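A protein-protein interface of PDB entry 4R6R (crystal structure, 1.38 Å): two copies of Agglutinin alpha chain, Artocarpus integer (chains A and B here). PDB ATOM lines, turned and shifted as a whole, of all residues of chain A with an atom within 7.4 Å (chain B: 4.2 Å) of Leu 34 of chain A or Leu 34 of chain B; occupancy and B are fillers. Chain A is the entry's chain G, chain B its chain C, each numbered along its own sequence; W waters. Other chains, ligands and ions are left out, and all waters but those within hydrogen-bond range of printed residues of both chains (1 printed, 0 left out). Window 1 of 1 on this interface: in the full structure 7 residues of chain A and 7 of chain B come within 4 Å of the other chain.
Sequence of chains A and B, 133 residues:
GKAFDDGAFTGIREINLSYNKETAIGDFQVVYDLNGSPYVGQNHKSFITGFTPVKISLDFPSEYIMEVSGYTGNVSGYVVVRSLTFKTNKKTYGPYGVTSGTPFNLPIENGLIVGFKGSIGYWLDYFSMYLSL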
ATOM      1  N   ASP A   6      18.750 -13.742  -5.009  1.00  0.00           N
ATOM      2  CA  ASP A   6      17.502 -13.368  -4.289  1.00  0.00           C
ATOM      3  C   ASP A   6      17.342 -14.157  -3.014  1.00  0.00           C
ATOM      4  O   ASP A   6      16.633 -13.687  -2.079  1.00  0.00           O
ATOM      5  CB  ASP A   6      16.248 -13.592  -5.165  1.00  0.00           C
ATOM      6  CG  ASP A   6      16.137 -12.594  -6.340  1.00  0.00           C
ATOM      7  OD1 ASP A   6      16.805 -11.547  -6.309  1.00  0.00           O
ATOM      8  OD2 ASP A   6      15.395 -12.933  -7.240  1.00  0.00           O
ATOM      9  N   GLY A   7      17.952 -15.333  -2.962  1.00  0.00           N
ATOM     10  CA  GLY A   7      17.728 -16.236  -1.840  1.00  0.00           C
ATOM     11  C   GLY A   7      16.523 -17.163  -2.076  1.00  0.00           C
ATOM     12  O   GLY A   7      15.958 -17.222  -3.187  1.00  0.00           O
ATOM     13  N   ALA A   8      16.123 -17.837  -1.022  1.00  0.00           N
ATOM     14  CA  ALA A   8      15.010 -18.810  -1.083  1.00  0.00           C
ATOM     15  C   ALA A   8      13.769 -18.299  -0.367  1.00  0.00           C
ATOM     16  O   ALA A   8      13.836 -17.585   0.646  1.00  0.00           O
ATOM     17  CB  ALA A   8      15.449 -20.123  -0.371  1.00  0.00           C
ATOM     18  N   PHE A   9      12.640 -18.661  -0.951  1.00  0.00           N
ATOM     19  CA  PHE A   9      11.305 -18.218  -0.501  1.00  0.00           C
ATOM     20  C   PHE A   9      10.364 -19.401  -0.399  1.00  0.00           C
ATOM     21  O   PHE A   9      10.801 -20.564  -0.363  1.00  0.00           O
ATOM     22  CB  PHE A   9      10.792 -17.163  -1.512  1.00  0.00           C
ATOM     23  CG  PHE A   9      11.663 -15.950  -1.532  1.00  0.00           C
ATOM     24  CD1 PHE A   9      12.798 -15.892  -2.326  1.00  0.00           C
ATOM     25  CD2 PHE A   9      11.390 -14.842  -0.706  1.00  0.00           C
ATOM     26  CE1 PHE A   9      13.683 -14.818  -2.306  1.00  0.00           C
ATOM     27  CE2 PHE A   9      12.282 -13.777  -0.693  1.00  0.00           C
ATOM     28  CZ  PHE A   9      13.396 -13.755  -1.516  1.00  0.00           C
ATOM     29  N   THR A  10       9.051 -19.150  -0.396  1.00  0.00           N
ATOM     30  CA  THR A  10       8.053 -20.227  -0.252  1.00  0.00           C
ATOM     31  C   THR A  10       7.527 -20.726  -1.573  1.00  0.00           C
ATOM     32  O   THR A  10       6.849 -21.738  -1.623  1.00  0.00           O
ATOM     33  CB  THR A  10       6.859 -19.714   0.645  1.00  0.00           C
ATOM     34  OG1 THR A  10       7.379 -18.860   1.667  1.00  0.00           O
ATOM     35  CG2 THR A  10       6.147 -20.900   1.319  1.00  0.00           C
ATOM     36  N   GLY A  11       7.801 -20.025  -2.677  1.00  0.00           N
ATOM     37  CA  GLY A  11       7.210 -20.318  -3.963  1.00  0.00           C
ATOM     38  C   GLY A  11       7.385 -19.150  -4.900  1.00  0.00           C
ATOM     39  O   GLY A  11       8.076 -18.191  -4.593  1.00  0.00           O
ATOM     40  N   ILE A  12       6.765 -19.307  -6.070  1.00  0.00           N
ATOM     41  CA  ILE A  12       6.877 -18.296  -7.146  1.00  0.00           C
ATOM     42  C   ILE A  12       5.488 -17.836  -7.539  1.00  0.00           C
ATOM     43  O   ILE A  12       4.611 -18.642  -7.875  1.00  0.00           O
ATOM     44  CB  ILE A  12       7.633 -18.870  -8.371  1.00  0.00           C
ATOM     45  CG1 ILE A  12       9.091 -19.169  -7.944  1.00  0.00           C
ATOM     46  CG2 ILE A  12       7.640 -17.859  -9.546  1.00  0.00           C
ATOM     47  CD1 ILE A  12       9.873 -19.875  -8.979  1.00  0.00           C
ATOM     48  N   ARG A  13       5.310 -16.511  -7.557  1.00  0.00           N
ATOM     49  CA  ARG A  13       4.054 -15.928  -8.083  1.00  0.00           C
ATOM     50  C   ARG A  13       4.166 -15.349  -9.487  1.00  0.00           C
ATOM     51  O   ARG A  13       3.225 -15.503 -10.273  1.00  0.00           O
ATOM     52  CB  ARG A  13       3.615 -14.828  -7.166  1.00  0.00           C
ATOM     53  CG  ARG A  13       3.039 -15.383  -5.876  1.00  0.00           C
ATOM     54  CD  ARG A  13       3.036 -14.348  -4.744  1.00  0.00           C
ATOM     55  NE  ARG A  13       2.268 -14.839  -3.580  1.00  0.00           N
ATOM     56  CZ  ARG A  13       0.933 -14.765  -3.436  1.00  0.00           C
ATOM     57  NH1 ARG A  13       0.126 -14.274  -4.377  1.00  0.00           N
ATOM     58  NH2 ARG A  13       0.439 -15.194  -2.294  1.00  0.00           N
ATOM     59  N   VAL A  31       8.538 -12.073  -8.506  1.00  0.00           N
ATOM     60  CA  VAL A  31       7.673 -11.932  -7.345  1.00  0.00           C
ATOM     61  C   VAL A  31       7.508 -13.329  -6.774  1.00  0.00           C
ATOM     62  O   VAL A  31       6.914 -14.210  -7.350  1.00  0.00           O
ATOM     63  CB  VAL A  31       6.294 -11.337  -7.681  1.00  0.00           C
ATOM     64  CG1 VAL A  31       5.523 -11.100  -6.367  1.00  0.00           C
ATOM     65  CG2 VAL A  31       6.436 -10.003  -8.424  1.00  0.00           C
ATOM     66  N   TYR A  32       8.134 -13.533  -5.601  1.00  0.00           N
ATOM     67  CA  TYR A  32       8.106 -14.751  -4.860  1.00  0.00           C
ATOM     68  C   TYR A  32       6.830 -14.831  -4.013  1.00  0.00           C
ATOM     69  O   TYR A  32       6.181 -13.791  -3.776  1.00  0.00           O
ATOM     70  CB  TYR A  32       9.364 -14.882  -3.935  1.00  0.00           C
ATOM     71  CG  TYR A  32      10.630 -14.950  -4.741  1.00  0.00           C
ATOM     72  CD1 TYR A  32      11.014 -16.186  -5.287  1.00  0.00           C
ATOM     73  CD2 TYR A  32      11.431 -13.854  -4.921  1.00  0.00           C
ATOM     74  CE1 TYR A  32      12.135 -16.266  -6.058  1.00  0.00           C
ATOM     75  CE2 TYR A  32      12.564 -13.915  -5.739  1.00  0.00           C
ATOM     76  CZ  TYR A  32      12.936 -15.157  -6.272  1.00  0.00           C
ATOM     77  OH  TYR A  32      14.091 -15.199  -7.045  1.00  0.00           O
ATOM     78  N   ASP A  33       6.499 -16.021  -3.564  1.00  0.00           N
ATOM     79  CA  ASP A  33       5.616 -16.146  -2.384  1.00  0.00           C
ATOM     80  C   ASP A  33       6.440 -16.227  -1.153  1.00  0.00           C
ATOM     81  O   ASP A  33       7.454 -16.955  -1.155  1.00  0.00           O
ATOM     82  CB  ASP A  33       4.687 -17.337  -2.474  1.00  0.00           C
ATOM     83  CG  ASP A  33       3.728 -17.332  -1.337  1.00  0.00           C
ATOM     84  OD1 ASP A  33       2.786 -16.515  -1.373  1.00  0.00           O
ATOM     85  OD2 ASP A  33       3.975 -18.062  -0.325  1.00  0.00           O
ATOM     86  N   LEU A  34       6.073 -15.459  -0.131  1.00  0.00           N
ATOM     87  CA  LEU A  34       6.740 -15.581   1.201  1.00  0.00           C
ATOM     88  C   LEU A  34       5.619 -15.841   2.199  1.00  0.00           C
ATOM     89  O   LEU A  34       4.901 -14.894   2.597  1.00  0.00           O
ATOM     90  CB  LEU A  34       7.578 -14.359   1.555  1.00  0.00           C
ATOM     91  CG  LEU A  34       8.283 -14.414   2.926  1.00  0.00           C
ATOM     92  CD1 LEU A  34       9.268 -15.594   2.932  1.00  0.00           C
ATOM     93  CD2 LEU A  34       8.938 -13.083   3.306  1.00  0.00           C
ATOM     94  N   ASN A  35       5.500 -17.106   2.578  1.00  0.00           N
ATOM     95  CA  ASN A  35       4.495 -17.485   3.585  1.00  0.00           C
ATOM     96  C   ASN A  35       3.133 -16.937   3.306  1.00  0.00           C
ATOM     97  O   ASN A  35       2.437 -16.475   4.205  1.00  0.00           O
ATOM     98  CB  ASN A  35       5.015 -17.025   4.937  1.00  0.00           C
ATOM     99  CG  ASN A  35       6.344 -17.671   5.250  1.00  0.00           C
ATOM    100  OD1 ASN A  35       6.505 -18.887   5.033  1.00  0.00           O
ATOM    101  ND2 ASN A  35       7.318 -16.895   5.702  1.00  0.00           N
ATOM    102  N   GLY A  36       2.765 -16.997   2.061  1.00  0.00           N
ATOM    103  CA  GLY A  36       1.383 -16.693   1.648  1.00  0.00           C
ATOM    104  C   GLY A  36       1.205 -15.318   1.084  1.00  0.00           C
ATOM    105  O   GLY A  36       0.127 -15.062   0.508  1.00  0.00           O
ATOM    106  N   SER A  37       2.219 -14.469   1.201  1.00  0.00           N
ATOM    107  CA  SER A  37       2.184 -13.116   0.663  1.00  0.00           C
ATOM    108  C   SER A  37       3.188 -12.879  -0.450  1.00  0.00           C
ATOM    109  O   SER A  37       4.245 -13.485  -0.467  1.00  0.00           O
ATOM    110  CB  SER A  37       2.467 -12.103   1.727  1.00  0.00           C
ATOM    111  OG  SER A  37       1.401 -12.196   2.701  1.00  0.00           O
ATOM    112  N   PRO A  38       2.881 -11.964  -1.366  1.00  0.00           N
ATOM    113  CA  PRO A  38       3.841 -11.648  -2.433  1.00  0.00           C
ATOM    114  C   PRO A  38       5.057 -10.974  -1.912  1.00  0.00           C
ATOM    115  O   PRO A  38       4.921 -10.064  -1.108  1.00  0.00           O
ATOM    116  CB  PRO A  38       3.074 -10.697  -3.363  1.00  0.00           C
ATOM    117  CG  PRO A  38       1.633 -10.922  -3.003  1.00  0.00           C
ATOM    118  CD  PRO A  38       1.583 -11.276  -1.561  1.00  0.00           C
ATOM    119  N   TYR A  39       6.240 -11.405  -2.356  1.00  0.00           N
ATOM    120  CA  TYR A  39       7.496 -10.728  -2.044  1.00  0.00           C
ATOM    121  C   TYR A  39       8.115 -10.222  -3.327  1.00  0.00           C
ATOM    122  O   TYR A  39       8.455 -11.024  -4.197  1.00  0.00           O
ATOM    123  CB  TYR A  39       8.446 -11.737  -1.357  1.00  0.00           C
ATOM    124  CG  TYR A  39       9.790 -11.113  -0.943  1.00  0.00           C
ATOM    125  CD1 TYR A  39      10.770 -10.808  -1.884  1.00  0.00           C
ATOM    126  CD2 TYR A  39      10.061 -10.830   0.403  1.00  0.00           C
ATOM    127  CE1 TYR A  39      11.987 -10.254  -1.473  1.00  0.00           C
ATOM    128  CE2 TYR A  39      11.243 -10.307   0.777  1.00  0.00           C
ATOM    129  CZ  TYR A  39      12.156 -10.002  -0.169  1.00  0.00           C
ATOM    130  OH  TYR A  39      13.377  -9.426   0.292  1.00  0.00           O
ATOM    131  N   PHE A  60      -0.809 -18.941  -8.495  1.00  0.00           N
ATOM    132  CA  PHE A  60      -0.263 -19.487  -7.248  1.00  0.00           C
ATOM    133  C   PHE A  60      -1.363 -19.682  -6.185  1.00  0.00           C
ATOM    134  O   PHE A  60      -2.234 -18.798  -6.007  1.00  0.00           O
ATOM    135  CB  PHE A  60       0.812 -18.507  -6.700  1.00  0.00           C
ATOM    136  CG  PHE A  60       1.380 -18.916  -5.387  1.00  0.00           C
ATOM    137  CD1 PHE A  60       2.437 -19.826  -5.327  1.00  0.00           C
ATOM    138  CD2 PHE A  60       0.840 -18.462  -4.182  1.00  0.00           C
ATOM    139  CE1 PHE A  60       2.962 -20.246  -4.113  1.00  0.00           C
ATOM    140  CE2 PHE A  60       1.344 -18.893  -2.973  1.00  0.00           C
ATOM    141  CZ  PHE A  60       2.433 -19.789  -2.925  1.00  0.00           C
ATOM    142  N   PHE B   9      11.320 -18.847   7.708  1.00  0.00           N
ATOM    143  CA  PHE B   9      12.360 -17.908   7.311  1.00  0.00           C
ATOM    144  C   PHE B   9      13.742 -18.577   7.281  1.00  0.00           C
ATOM    145  O   PHE B   9      13.816 -19.794   7.224  1.00  0.00           O
ATOM    146  CB  PHE B   9      12.324 -16.693   8.242  1.00  0.00           C
ATOM    147  CG  PHE B   9      11.066 -15.947   8.141  1.00  0.00           C
ATOM    148  CD1 PHE B   9       9.959 -16.329   8.891  1.00  0.00           C
ATOM    149  CD2 PHE B   9      10.947 -14.866   7.254  1.00  0.00           C
ATOM    150  CE1 PHE B   9       8.750 -15.686   8.782  1.00  0.00           C
ATOM    151  CE2 PHE B   9       9.730 -14.209   7.155  1.00  0.00           C
ATOM    152  CZ  PHE B   9       8.635 -14.588   7.904  1.00  0.00           C
ATOM    153  N   THR B  10      14.833 -17.810   7.187  1.00  0.00           N
ATOM    154  CA  THR B  10      16.196 -18.360   7.134  1.00  0.00           C
ATOM    155  C   THR B  10      16.850 -18.544   8.505  1.00  0.00           C
ATOM    156  O   THR B  10      17.775 -19.240   8.588  1.00  0.00           O
ATOM    157  CB  THR B  10      17.178 -17.374   6.358  1.00  0.00           C
ATOM    158  OG1 THR B  10      16.532 -16.848   5.217  1.00  0.00           O
ATOM    159  CG2 THR B  10      18.470 -18.050   5.965  1.00  0.00           C
ATOM    160  N   TYR B  32      13.210 -12.048  12.134  1.00  0.00           N
ATOM    161  CA  TYR B  32      13.825 -13.174  11.441  1.00  0.00           C
ATOM    162  C   TYR B  32      15.009 -12.758  10.592  1.00  0.00           C
ATOM    163  O   TYR B  32      15.187 -11.552  10.332  1.00  0.00           O
ATOM    164  CB  TYR B  32      12.745 -13.851  10.511  1.00  0.00           C
ATOM    165  CG  TYR B  32      11.618 -14.506  11.255  1.00  0.00           C
ATOM    166  CD1 TYR B  32      11.852 -15.754  11.916  1.00  0.00           C
ATOM    167  CD2 TYR B  32      10.407 -13.862  11.473  1.00  0.00           C
ATOM    168  CE1 TYR B  32      10.837 -16.357  12.615  1.00  0.00           C
ATOM    169  CE2 TYR B  32       9.378 -14.475  12.207  1.00  0.00           C
ATOM    170  CZ  TYR B  32       9.603 -15.744  12.758  1.00  0.00           C
ATOM    171  OH  TYR B  32       8.635 -16.341  13.480  1.00  0.00           O
ATOM    172  N   ASP B  33      15.828 -13.718  10.205  1.00  0.00           N
ATOM    173  CA  ASP B  33      16.699 -13.517   9.076  1.00  0.00           C
ATOM    174  C   ASP B  33      15.952 -13.996   7.835  1.00  0.00           C
ATOM    175  O   ASP B  33      15.289 -15.032   7.876  1.00  0.00           O
ATOM    176  CB  ASP B  33      17.955 -14.339   9.222  1.00  0.00           C
ATOM    177  CG  ASP B  33      18.932 -14.044   8.102  1.00  0.00           C
ATOM    178  OD1 ASP B  33      19.417 -12.898   8.042  1.00  0.00           O
ATOM    179  OD2 ASP B  33      19.111 -14.935   7.229  1.00  0.00           O
ATOM    180  N   LEU B  34      16.063 -13.281   6.713  1.00  0.00           N
ATOM    181  CA  LEU B  34      15.498 -13.764   5.465  1.00  0.00           C
ATOM    182  C   LEU B  34      16.616 -13.534   4.432  1.00  0.00           C
ATOM    183  O   LEU B  34      16.841 -12.402   4.016  1.00  0.00           O
ATOM    184  CB  LEU B  34      14.251 -12.980   5.101  1.00  0.00           C
ATOM    185  CG  LEU B  34      13.633 -13.335   3.728  1.00  0.00           C
ATOM    186  CD1 LEU B  34      13.127 -14.767   3.729  1.00  0.00           C
ATOM    187  CD2 LEU B  34      12.471 -12.425   3.447  1.00  0.00           C
ATOM    188  N   ASN B  35      17.317 -14.603   4.132  1.00  0.00           N
ATOM    189  CA  ASN B  35      18.379 -14.657   3.120  1.00  0.00           C
ATOM    190  C   ASN B  35      19.462 -13.627   3.421  1.00  0.00           C
ATOM    191  O   ASN B  35      19.901 -12.924   2.534  1.00  0.00           O
ATOM    192  CB  ASN B  35      17.730 -14.451   1.736  1.00  0.00           C
ATOM    193  CG  ASN B  35      16.723 -15.543   1.418  1.00  0.00           C
ATOM    194  OD1 ASN B  35      15.585 -15.226   1.012  1.00  0.00           O
ATOM    195  ND2 ASN B  35      17.143 -16.770   1.502  1.00  0.00           N
ATOM    196  N   GLY B  36      19.857 -13.568   4.704  1.00  0.00           N
ATOM    197  CA  GLY B  36      20.956 -12.702   5.202  1.00  0.00           C
ATOM    198  C   GLY B  36      20.552 -11.257   5.519  1.00  0.00           C
ATOM    199  O   GLY B  36      21.405 -10.410   5.850  1.00  0.00           O
ATOM    200  N   SER B  37      19.286 -10.928   5.391  1.00  0.00           N
ATOM    201  CA  SER B  37      18.761  -9.586   5.742  1.00  0.00           C
ATOM    202  C   SER B  37      17.660  -9.659   6.824  1.00  0.00           C
ATOM    203  O   SER B  37      16.952 -10.652   6.901  1.00  0.00           O
ATOM    204  CB  SER B  37      18.174  -8.918   4.514  1.00  0.00           C
ATOM    205  OG  SER B  37      19.250  -8.485   3.694  1.00  0.00           O
ATOM    206  N   TYR B  39      14.145  -9.399   8.633  1.00  0.00           N
ATOM    207  CA  TYR B  39      12.767  -9.319   8.280  1.00  0.00           C
ATOM    208  C   TYR B  39      11.985  -9.169   9.578  1.00  0.00           C
ATOM    209  O   TYR B  39      12.039 -10.080  10.493  1.00  0.00           O
ATOM    210  CB  TYR B  39      12.304 -10.573   7.539  1.00  0.00           C
ATOM    211  CG  TYR B  39      10.863 -10.493   7.164  1.00  0.00           C
ATOM    212  CD1 TYR B  39       9.843 -10.913   8.031  1.00  0.00           C
ATOM    213  CD2 TYR B  39      10.500  -9.966   5.920  1.00  0.00           C
ATOM    214  CE1 TYR B  39       8.512 -10.844   7.675  1.00  0.00           C
ATOM    215  CE2 TYR B  39       9.186  -9.875   5.572  1.00  0.00           C
ATOM    216  CZ  TYR B  39       8.206 -10.306   6.423  1.00  0.00           C
ATOM    217  OH  TYR B  39       6.906 -10.201   6.013  1.00  0.00           O
HETATM  218  O   HOH W   1      15.236 -11.821   0.726  1.00  0.00           O
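Among the printed residues, merely in contact across the chains: Gly 7 of chain A with Asn 35 of chain B, Asn 35 of chain A with Phe 9 of chain B, Leu 34 of chain A with Leu 34 of chain B, Asp 6 of chain A with Asn 35 of chain B, Tyr 39 of chain A with Leu 34 of chain B, Phe 9 of chain A with Asn 35 of chain B and Leu 34 of chain A with Tyr 39 of chain B.
Water W1 lies within hydrogen-bond range of OH of Tyr 39 of chain A (3.1 Å) and OD1 of Asn 35 of chain B (3.4 Å).
The backbone NH (N) of Asn 35 of chain B sits at hydrogen-bond distance from the side-chain hydroxyl (OG1) of Thr 10 of chain B (2.6 Å). The backbone NH (N) of Tyr 32 of chain B lies within hydrogen-bond range of the backbone carbonyl oxygen (O) of Tyr 39 of chain B, 2.8 Å away. OD2 of Asp 6 of chain A is in hydrogen-bond range of OH of Tyr 32 of chain A, 2.6 Å away. N of Asn 35 of chain A sits at hydrogen-bond distance from OG1 of Thr 10 of chain A, at 2.7 Å. The backbone carbonyl oxygen of Tyr 32 of chain A lies within hydrogen-bond range of the backbone NH of Tyr 39 of chain A, at 2.8 Å. The side-chain carboxylate of Asp 33 of chain A sits at hydrogen-bond distance from the backbone NH of Asn 35 of chain A.
Hydrophobic or aromatic side chains of chain A that line the printed part of chain B: Phe 9, Leu 34 and Tyr 39. Of the 9 printed residues of chain B, 4 touch a printed residue of chain A. Hydrophobic or aromatic side chains of chain B that line the printed part of chain A: Phe 9, Leu 34 and Tyr 39. Among the printed residues, no Asp or Glu carboxylate lies within 4 Å of a Lys or Arg side-chain nitrogen of the other chain.
Of the printed residues of chain B, Asp 6 of chain A touches Asn 35 (3.6 Å). Of the printed residues of chain B, Gly 7 of chain A touches Asn 35. Printed residues of chain B within 4 Å of Phe 9 of chain A: Asn 35. Printed residues of chain B within 4 Å of Leu 34 of chain A: Leu 34 (3.6 Å) and Tyr 39 (3.9 Å). Ser 37 of chain A touches none of the printed residues of chain B. Of the printed residues of chain B, Tyr 39 of chain A touches Leu 34. Leu 34 of chain B touches just these residues of chain A: Leu 34 (3.6 Å) and Tyr 39 (3.6 Å). The nearest residue of chain B that does not touch Leu 34 of chain A is Phe 9 of chain B (4.1 Å). The nearest residue of chain A that does not touch Leu 34 of chain B is Ala 8 of chain A (4.2 Å).
N of Ala 8 of chain A sits close to ND2 of Asn 35 of chain B, at 2.9 Å.
Phe 9 of chain A touches Asn 35 of chain B, and with the chains exchanged Asn 35 of chain A touches Phe 9 of chain B. Leu 34 of chain B touches its own counterpart, Leu 34 of chain A. Leu 34 of chain A touches Tyr 39 of chain B, and with the chains exchanged Tyr 39 of chain A touches Leu 34 of chain B. Positions printed for both chains: 9, 10, 32, 33, 34, 35, 36, 37 and 39. Of the 8 pairs that touch across the chains among the printed residues, 5 have their exchanged pair printed and touching as well.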
